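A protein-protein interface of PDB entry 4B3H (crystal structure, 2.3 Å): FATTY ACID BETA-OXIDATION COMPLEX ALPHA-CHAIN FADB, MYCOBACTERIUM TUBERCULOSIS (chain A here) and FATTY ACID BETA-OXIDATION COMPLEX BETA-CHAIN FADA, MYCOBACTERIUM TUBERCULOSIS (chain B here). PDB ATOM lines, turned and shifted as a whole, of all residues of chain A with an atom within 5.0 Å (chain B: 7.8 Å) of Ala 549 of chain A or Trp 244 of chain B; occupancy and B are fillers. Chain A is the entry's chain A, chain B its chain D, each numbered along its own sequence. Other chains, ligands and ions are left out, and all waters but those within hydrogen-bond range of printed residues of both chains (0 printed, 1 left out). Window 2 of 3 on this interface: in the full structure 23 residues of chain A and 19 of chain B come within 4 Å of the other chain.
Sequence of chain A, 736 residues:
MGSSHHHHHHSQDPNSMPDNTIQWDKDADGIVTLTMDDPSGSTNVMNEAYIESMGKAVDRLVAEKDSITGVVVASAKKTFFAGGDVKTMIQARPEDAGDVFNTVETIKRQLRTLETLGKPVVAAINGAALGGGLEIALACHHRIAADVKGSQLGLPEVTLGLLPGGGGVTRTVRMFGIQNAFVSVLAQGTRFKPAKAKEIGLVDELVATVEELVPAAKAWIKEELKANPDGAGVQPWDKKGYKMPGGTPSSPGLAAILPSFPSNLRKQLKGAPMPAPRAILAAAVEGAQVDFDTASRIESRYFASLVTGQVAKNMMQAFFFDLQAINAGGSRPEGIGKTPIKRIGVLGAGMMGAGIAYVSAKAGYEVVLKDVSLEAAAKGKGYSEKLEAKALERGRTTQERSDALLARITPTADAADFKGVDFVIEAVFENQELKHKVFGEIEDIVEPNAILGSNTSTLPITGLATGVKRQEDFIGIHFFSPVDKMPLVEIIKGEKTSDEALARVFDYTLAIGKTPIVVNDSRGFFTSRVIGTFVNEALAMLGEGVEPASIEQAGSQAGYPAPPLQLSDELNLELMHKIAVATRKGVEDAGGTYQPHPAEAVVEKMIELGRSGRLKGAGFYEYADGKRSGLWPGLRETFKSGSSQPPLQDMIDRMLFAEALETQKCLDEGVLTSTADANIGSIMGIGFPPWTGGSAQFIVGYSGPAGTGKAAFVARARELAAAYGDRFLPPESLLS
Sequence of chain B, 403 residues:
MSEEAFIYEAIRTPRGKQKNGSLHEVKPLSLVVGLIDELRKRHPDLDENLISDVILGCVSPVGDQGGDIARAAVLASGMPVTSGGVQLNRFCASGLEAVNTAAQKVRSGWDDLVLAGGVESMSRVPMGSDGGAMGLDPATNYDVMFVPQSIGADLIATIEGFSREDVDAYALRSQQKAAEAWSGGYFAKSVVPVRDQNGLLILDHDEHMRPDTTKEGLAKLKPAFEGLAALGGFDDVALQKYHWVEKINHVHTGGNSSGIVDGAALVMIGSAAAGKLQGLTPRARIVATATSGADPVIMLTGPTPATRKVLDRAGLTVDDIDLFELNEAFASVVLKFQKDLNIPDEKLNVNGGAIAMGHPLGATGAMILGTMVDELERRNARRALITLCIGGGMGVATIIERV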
ATOM      1  N   GLU A 547     -17.518  33.152  27.777  1.00  0.00           N
ATOM      2  CA  GLU A 547     -17.251  33.105  26.335  1.00  0.00           C
ATOM      3  C   GLU A 547     -17.840  31.848  25.686  1.00  0.00           C
ATOM      4  O   GLU A 547     -17.610  30.735  26.172  1.00  0.00           O
ATOM      5  CB  GLU A 547     -15.744  33.167  26.058  1.00  0.00           C
ATOM      6  CG  GLU A 547     -15.089  34.514  26.347  1.00  0.00           C
ATOM      7  CD  GLU A 547     -15.249  35.529  25.224  1.00  0.00           C
ATOM      8  OE1 GLU A 547     -16.107  35.337  24.334  1.00  0.00           O
ATOM      9  OE2 GLU A 547     -14.508  36.535  25.230  1.00  0.00           O
ATOM     10  N   PRO A 548     -18.617  32.023  24.599  1.00  0.00           N
ATOM     11  CA  PRO A 548     -19.178  30.893  23.858  1.00  0.00           C
ATOM     12  C   PRO A 548     -18.117  29.897  23.397  1.00  0.00           C
ATOM     13  O   PRO A 548     -18.329  28.687  23.508  1.00  0.00           O
ATOM     14  CB  PRO A 548     -19.843  31.558  22.647  1.00  0.00           C
ATOM     15  CG  PRO A 548     -20.199  32.921  23.120  1.00  0.00           C
ATOM     16  CD  PRO A 548     -19.136  33.315  24.108  1.00  0.00           C
ATOM     17  N   ALA A 549     -16.992  30.403  22.890  1.00  0.00           N
ATOM     18  CA  ALA A 549     -15.893  29.557  22.423  1.00  0.00           C
ATOM     19  C   ALA A 549     -15.353  28.656  23.539  1.00  0.00           C
ATOM     20  O   ALA A 549     -14.998  27.502  23.291  1.00  0.00           O
ATOM     21  CB  ALA A 549     -14.777  30.404  21.830  1.00  0.00           C
ATOM     22  N   SER A 550     -15.305  29.188  24.761  1.00  0.00           N
ATOM     23  CA  SER A 550     -14.867  28.424  25.935  1.00  0.00           C
ATOM     24  C   SER A 550     -15.868  27.336  26.301  1.00  0.00           C
ATOM     25  O   SER A 550     -15.475  26.207  26.607  1.00  0.00           O
ATOM     26  CB  SER A 550     -14.638  29.344  27.140  1.00  0.00           C
ATOM     27  OG  SER A 550     -13.493  30.155  26.958  1.00  0.00           O
ATOM     28  N   ILE A 551     -17.154  27.686  26.269  1.00  0.00           N
ATOM     29  CA  ILE A 551     -18.239  26.747  26.555  1.00  0.00           C
ATOM     30  C   ILE A 551     -18.178  25.548  25.610  1.00  0.00           C
ATOM     31  O   ILE A 551     -18.316  24.396  26.044  1.00  0.00           O
ATOM     32  CB  ILE A 551     -19.624  27.432  26.466  1.00  0.00           C
ATOM     33  CG1 ILE A 551     -19.760  28.499  27.556  1.00  0.00           C
ATOM     34  CG2 ILE A 551     -20.747  26.409  26.591  1.00  0.00           C
ATOM     35  CD1 ILE A 551     -20.949  29.424  27.385  1.00  0.00           C
ATOM     36  N   GLU A 552     -17.950  25.827  24.326  1.00  0.00           N
ATOM     37  CA  GLU A 552     -17.857  24.783  23.308  1.00  0.00           C
ATOM     38  C   GLU A 552     -16.628  23.908  23.518  1.00  0.00           C
ATOM     39  O   GLU A 552     -16.715  22.680  23.441  1.00  0.00           O
ATOM     40  CB  GLU A 552     -17.886  25.380  21.893  1.00  0.00           C
ATOM     41  CG  GLU A 552     -19.188  26.087  21.527  1.00  0.00           C
ATOM     42  CD  GLU A 552     -20.412  25.191  21.646  1.00  0.00           C
ATOM     43  OE1 GLU A 552     -20.824  24.879  22.786  1.00  0.00           O
ATOM     44  OE2 GLU A 552     -20.967  24.787  20.600  1.00  0.00           O
ATOM     45  N   GLN A 553     -15.495  24.548  23.807  1.00  0.00           N
ATOM     46  CA  GLN A 553     -14.259  23.844  24.146  1.00  0.00           C
ATOM     47  C   GLN A 553     -14.418  22.954  25.375  1.00  0.00           C
ATOM     48  O   GLN A 553     -13.937  21.821  25.393  1.00  0.00           O
ATOM     49  CB  GLN A 553     -13.120  24.838  24.375  1.00  0.00           C
ATOM     50  CG  GLN A 553     -12.386  25.251  23.110  1.00  0.00           C
ATOM     51  CD  GLN A 553     -11.584  24.119  22.486  1.00  0.00           C
ATOM     52  OE1 GLN A 553     -11.219  23.144  23.152  1.00  0.00           O
ATOM     53  NE2 GLN A 553     -11.301  24.248  21.192  1.00  0.00           N
ATOM     54  N   LEU A 631     -20.007  30.539  15.107  1.00  0.00           N
ATOM     55  CA  LEU A 631     -20.772  31.154  16.191  1.00  0.00           C
ATOM     56  C   LEU A 631     -21.286  32.534  15.789  1.00  0.00           C
ATOM     57  O   LEU A 631     -20.552  33.332  15.198  1.00  0.00           O
ATOM     58  CB  LEU A 631     -19.936  31.253  17.472  1.00  0.00           C
ATOM     59  CG  LEU A 631     -19.706  29.980  18.296  1.00  0.00           C
ATOM     60  CD1 LEU A 631     -18.591  30.201  19.306  1.00  0.00           C
ATOM     61  CD2 LEU A 631     -20.980  29.531  18.999  1.00  0.00           C
ATOM     62  N   LEU B 155      -1.311  33.059  16.287  1.00  0.00           N
ATOM     63  CA  LEU B 155      -2.158  33.221  17.463  1.00  0.00           C
ATOM     64  C   LEU B 155      -1.951  34.589  18.117  1.00  0.00           C
ATOM     65  O   LEU B 155      -2.919  35.248  18.503  1.00  0.00           O
ATOM     66  CB  LEU B 155      -1.903  32.081  18.456  1.00  0.00           C
ATOM     67  CG  LEU B 155      -2.793  31.896  19.686  1.00  0.00           C
ATOM     68  CD1 LEU B 155      -4.267  31.771  19.328  1.00  0.00           C
ATOM     69  CD2 LEU B 155      -2.325  30.671  20.455  1.00  0.00           C
ATOM     70  N   ILE B 159      -4.985  37.343  18.661  1.00  0.00           N
ATOM     71  CA  ILE B 159      -5.330  37.940  19.956  1.00  0.00           C
ATOM     72  C   ILE B 159      -5.134  39.461  19.954  1.00  0.00           C
ATOM     73  O   ILE B 159      -6.037  40.205  20.336  1.00  0.00           O
ATOM     74  CB  ILE B 159      -4.539  37.278  21.114  1.00  0.00           C
ATOM     75  CG1 ILE B 159      -4.911  35.793  21.232  1.00  0.00           C
ATOM     76  CG2 ILE B 159      -4.793  37.996  22.438  1.00  0.00           C
ATOM     77  CD1 ILE B 159      -3.934  34.964  22.041  1.00  0.00           C
ATOM     78  N   ALA B 238      -3.648  24.140  19.929  1.00  0.00           N
ATOM     79  CA  ALA B 238      -3.443  25.510  20.394  1.00  0.00           C
ATOM     80  C   ALA B 238      -4.718  26.087  21.005  1.00  0.00           C
ATOM     81  O   ALA B 238      -4.675  26.719  22.066  1.00  0.00           O
ATOM     82  CB  ALA B 238      -2.947  26.392  19.257  1.00  0.00           C
ATOM     83  N   LEU B 239      -5.850  25.845  20.343  1.00  0.00           N
ATOM     84  CA  LEU B 239      -7.146  26.342  20.801  1.00  0.00           C
ATOM     85  C   LEU B 239      -7.711  25.563  21.995  1.00  0.00           C
ATOM     86  O   LEU B 239      -8.620  26.039  22.670  1.00  0.00           O
ATOM     87  CB  LEU B 239      -8.151  26.385  19.643  1.00  0.00           C
ATOM     88  CG  LEU B 239      -7.844  27.352  18.492  1.00  0.00           C
ATOM     89  CD1 LEU B 239      -8.856  27.203  17.366  1.00  0.00           C
ATOM     90  CD2 LEU B 239      -7.793  28.793  18.978  1.00  0.00           C
ATOM     91  N   GLN B 240      -7.172  24.375  22.255  1.00  0.00           N
ATOM     92  CA  GLN B 240      -7.529  23.632  23.462  1.00  0.00           C
ATOM     93  C   GLN B 240      -7.006  24.343  24.713  1.00  0.00           C
ATOM     94  O   GLN B 240      -7.689  24.376  25.741  1.00  0.00           O
ATOM     95  CB  GLN B 240      -7.024  22.187  23.400  1.00  0.00           C
ATOM     96  CG  GLN B 240      -7.907  21.260  22.572  1.00  0.00           C
ATOM     97  CD  GLN B 240      -7.329  19.861  22.402  1.00  0.00           C
ATOM     98  OE1 GLN B 240      -6.557  19.379  23.236  1.00  0.00           O
ATOM     99  NE2 GLN B 240      -7.715  19.198  21.317  1.00  0.00           N
ATOM    100  N   LYS B 241      -5.801  24.911  24.619  1.00  0.00           N
ATOM    101  CA  LYS B 241      -5.245  25.724  25.703  1.00  0.00           C
ATOM    102  C   LYS B 241      -5.880  27.109  25.729  1.00  0.00           C
ATOM    103  O   LYS B 241      -6.299  27.583  26.784  1.00  0.00           O
ATOM    104  CB  LYS B 241      -3.722  25.849  25.593  1.00  0.00           C
ATOM    105  CG  LYS B 241      -3.102  26.587  26.771  1.00  0.00           C
ATOM    106  CD  LYS B 241      -1.614  26.323  26.890  1.00  0.00           C
ATOM    107  CE  LYS B 241      -1.129  26.556  28.314  1.00  0.00           C
ATOM    108  NZ  LYS B 241       0.220  25.959  28.537  1.00  0.00           N
ATOM    109  N   TYR B 242      -5.944  27.745  24.562  1.00  0.00           N
ATOM    110  CA  TYR B 242      -6.539  29.072  24.419  1.00  0.00           C
ATOM    111  C   TYR B 242      -8.019  28.959  24.041  1.00  0.00           C
ATOM    112  O   TYR B 242      -8.438  29.366  22.950  1.00  0.00           O
ATOM    113  CB  TYR B 242      -5.737  29.907  23.410  1.00  0.00           C
ATOM    114  CG  TYR B 242      -4.371  30.294  23.933  1.00  0.00           C
ATOM    115  CD1 TYR B 242      -3.275  29.436  23.800  1.00  0.00           C
ATOM    116  CD2 TYR B 242      -4.179  31.509  24.584  1.00  0.00           C
ATOM    117  CE1 TYR B 242      -2.026  29.786  24.298  1.00  0.00           C
ATOM    118  CE2 TYR B 242      -2.939  31.870  25.085  1.00  0.00           C
ATOM    119  CZ  TYR B 242      -1.867  31.005  24.938  1.00  0.00           C
ATOM    120  OH  TYR B 242      -0.641  31.378  25.438  1.00  0.00           O
ATOM    121  N   HIS B 243      -8.801  28.411  24.973  1.00  0.00           N
ATOM    122  CA  HIS B 243     -10.204  28.053  24.732  1.00  0.00           C
ATOM    123  C   HIS B 243     -11.143  29.196  24.414  1.00  0.00           C
ATOM    124  O   HIS B 243     -12.190  28.985  23.801  1.00  0.00           O
ATOM    125  CB  HIS B 243     -10.751  27.180  25.863  1.00  0.00           C
ATOM    126  CG  HIS B 243     -10.512  27.732  27.249  1.00  0.00           C
ATOM    127  ND1 HIS B 243     -11.318  28.650  27.814  1.00  0.00           N
ATOM    128  CD2 HIS B 243      -9.532  27.436  28.195  1.00  0.00           C
ATOM    129  CE1 HIS B 243     -10.874  28.938  29.052  1.00  0.00           C
ATOM    130  NE2 HIS B 243      -9.781  28.195  29.284  1.00  0.00           N
ATOM    131  N   TRP B 244     -10.773  30.411  24.813  1.00  0.00           N
ATOM    132  CA  TRP B 244     -11.596  31.601  24.562  1.00  0.00           C
ATOM    133  C   TRP B 244     -11.449  32.154  23.165  1.00  0.00           C
ATOM    134  O   TRP B 244     -12.258  32.979  22.738  1.00  0.00           O
ATOM    135  CB  TRP B 244     -11.309  32.685  25.598  1.00  0.00           C
ATOM    136  CG  TRP B 244      -9.856  33.085  25.657  1.00  0.00           C
ATOM    137  CD1 TRP B 244      -9.221  34.091  24.934  1.00  0.00           C
ATOM    138  CD2 TRP B 244      -8.797  32.480  26.478  1.00  0.00           C
ATOM    139  NE1 TRP B 244      -7.886  34.153  25.248  1.00  0.00           N
ATOM    140  CE2 TRP B 244      -7.565  33.217  26.166  1.00  0.00           C
ATOM    141  CE3 TRP B 244      -8.748  31.448  27.408  1.00  0.00           C
ATOM    142  CZ2 TRP B 244      -6.351  32.915  26.771  1.00  0.00           C
ATOM    143  CZ3 TRP B 244      -7.518  31.150  28.012  1.00  0.00           C
ATOM    144  CH2 TRP B 244      -6.348  31.865  27.697  1.00  0.00           C
ATOM    145  N   VAL B 245     -10.420  31.710  22.446  1.00  0.00           N
ATOM    146  CA  VAL B 245     -10.210  32.101  21.049  1.00  0.00           C
ATOM    147  C   VAL B 245     -10.925  31.112  20.122  1.00  0.00           C
ATOM    148  O   VAL B 245     -10.708  29.906  20.216  1.00  0.00           O
ATOM    149  CB  VAL B 245      -8.705  32.158  20.686  1.00  0.00           C
ATOM    150  CG1 VAL B 245      -8.507  32.626  19.249  1.00  0.00           C
ATOM    151  CG2 VAL B 245      -7.948  33.064  21.647  1.00  0.00           C
ATOM    152  N   GLU B 246     -11.766  31.618  19.225  1.00  0.00           N
ATOM    153  CA  GLU B 246     -12.550  30.738  18.352  1.00  0.00           C
ATOM    154  C   GLU B 246     -11.779  30.227  17.130  1.00  0.00           C
ATOM    155  O   GLU B 246     -11.878  29.050  16.771  1.00  0.00           O
ATOM    156  CB  GLU B 246     -13.845  31.425  17.903  1.00  0.00           C
ATOM    157  CG  GLU B 246     -14.887  30.459  17.351  1.00  0.00           C
ATOM    158  CD  GLU B 246     -15.967  31.141  16.531  1.00  0.00           C
ATOM    159  OE1 GLU B 246     -16.149  32.369  16.678  1.00  0.00           O
ATOM    160  OE2 GLU B 246     -16.642  30.443  15.739  1.00  0.00           O
ATOM    161  N   LYS B 247     -11.017  31.119  16.499  1.00  0.00           N
ATOM    162  CA  LYS B 247     -10.395  30.845  15.208  1.00  0.00           C
ATOM    163  C   LYS B 247      -9.043  31.547  15.099  1.00  0.00           C
ATOM    164  O   LYS B 247      -8.935  32.742  15.375  1.00  0.00           O
ATOM    165  CB  LYS B 247     -11.340  31.305  14.085  1.00  0.00           C
ATOM    166  CG  LYS B 247     -10.743  31.398  12.685  1.00  0.00           C
ATOM    167  CD  LYS B 247     -10.756  30.063  11.949  1.00  0.00           C
ATOM    168  CE  LYS B 247     -11.097  30.240  10.474  1.00  0.00           C
ATOM    169  NZ  LYS B 247     -10.204  31.216   9.782  1.00  0.00           N
ATOM    170  N   ILE B 298       2.011  29.303  22.984  1.00  0.00           N
ATOM    171  CA  ILE B 298       2.137  30.534  22.195  1.00  0.00           C
ATOM    172  C   ILE B 298       3.613  30.747  21.818  1.00  0.00           C
ATOM    173  O   ILE B 298       3.922  31.346  20.785  1.00  0.00           O
ATOM    174  CB  ILE B 298       1.520  31.760  22.926  1.00  0.00           C
ATOM    175  CG1 ILE B 298       1.030  32.809  21.919  1.00  0.00           C
ATOM    176  CG2 ILE B 298       2.475  32.351  23.960  1.00  0.00           C
ATOM    177  CD1 ILE B 298       0.049  33.811  22.498  1.00  0.00           C
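A ring nitrogen (ND1) of His 243 of chain B sits at hydrogen-bond distance from the side-chain hydroxyl (OG) of Ser 550 of chain A (2.8 Å).
The side-chain hydroxyl of Ser 550 of chain A sits close to the backbone NH of Trp 244 of chain B (3.5 Å).
The backbone NH of Leu 631 of chain A lies within hydrogen-bond range of the side-chain carboxylate of Glu 246 of chain B.
The backbone carbonyl oxygen of Ala 549 of chain A sits close to the backbone carbonyl oxygen of His 243 of chain B, 3.2 Å away.
Ala 549 of chain A touches Trp 244 of chain B (CB to O, 3.7 Å).
O of Leu 239 of chain B touches CD of Gln 553 of chain A (3.5 Å).
Gln 553 of chain A touches Gln 240 of chain B (OE1 to CA, 3.7 Å).
His 243 of chain B touches Gln 553 of chain A (CB to CB, 3.6 Å).
Of chain A, only Ala 549 (3.7 Å) and Ser 550 (3.4 Å) come within 4 Å of Trp 244 of chain B.
Of the printed residues of chain B, Ser 550 of chain A touches His 243 (2.8 Å) and Trp 244 (3.4 Å).
Printed residues of chain B within 4 Å of Gln 553 of chain A: Leu 239 (3.5 Å), Gln 240 (3.7 Å) and His 243 (3.6 Å).
Printed residues of chain A within 4 Å of Glu 246 of chain B: Leu 631 (3.4 Å).
Printed residues of chain B within 4 Å of Leu 631 of chain A: Glu 246 (3.4 Å).
Tyr 242 of chain B touches none of the printed residues of chain A.
Pro 548 of chain A touches none of the printed residues of chain B.
Of the 13 printed residues of chain B, 5 touch a printed residue of chain A.
Printed residues of chain B that touch a printed residue of chain A: Leu 239, Gln 240, His 243, Trp 244 and Glu 246.
Hydrophobic or aromatic side chains of chain B within 4 Å of the printed part of chain A: His 243 and Trp 244.
Hydrophobic or aromatic side chains of chain A that line the printed part of chain B: Ala 549 and Leu 631.
Among the printed residues, 8 pairs touch across the chains.
Among the printed residues, no Asp or Glu carboxylate lies within 4 Å of a Lys or Arg side-chain nitrogen of the other chain.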
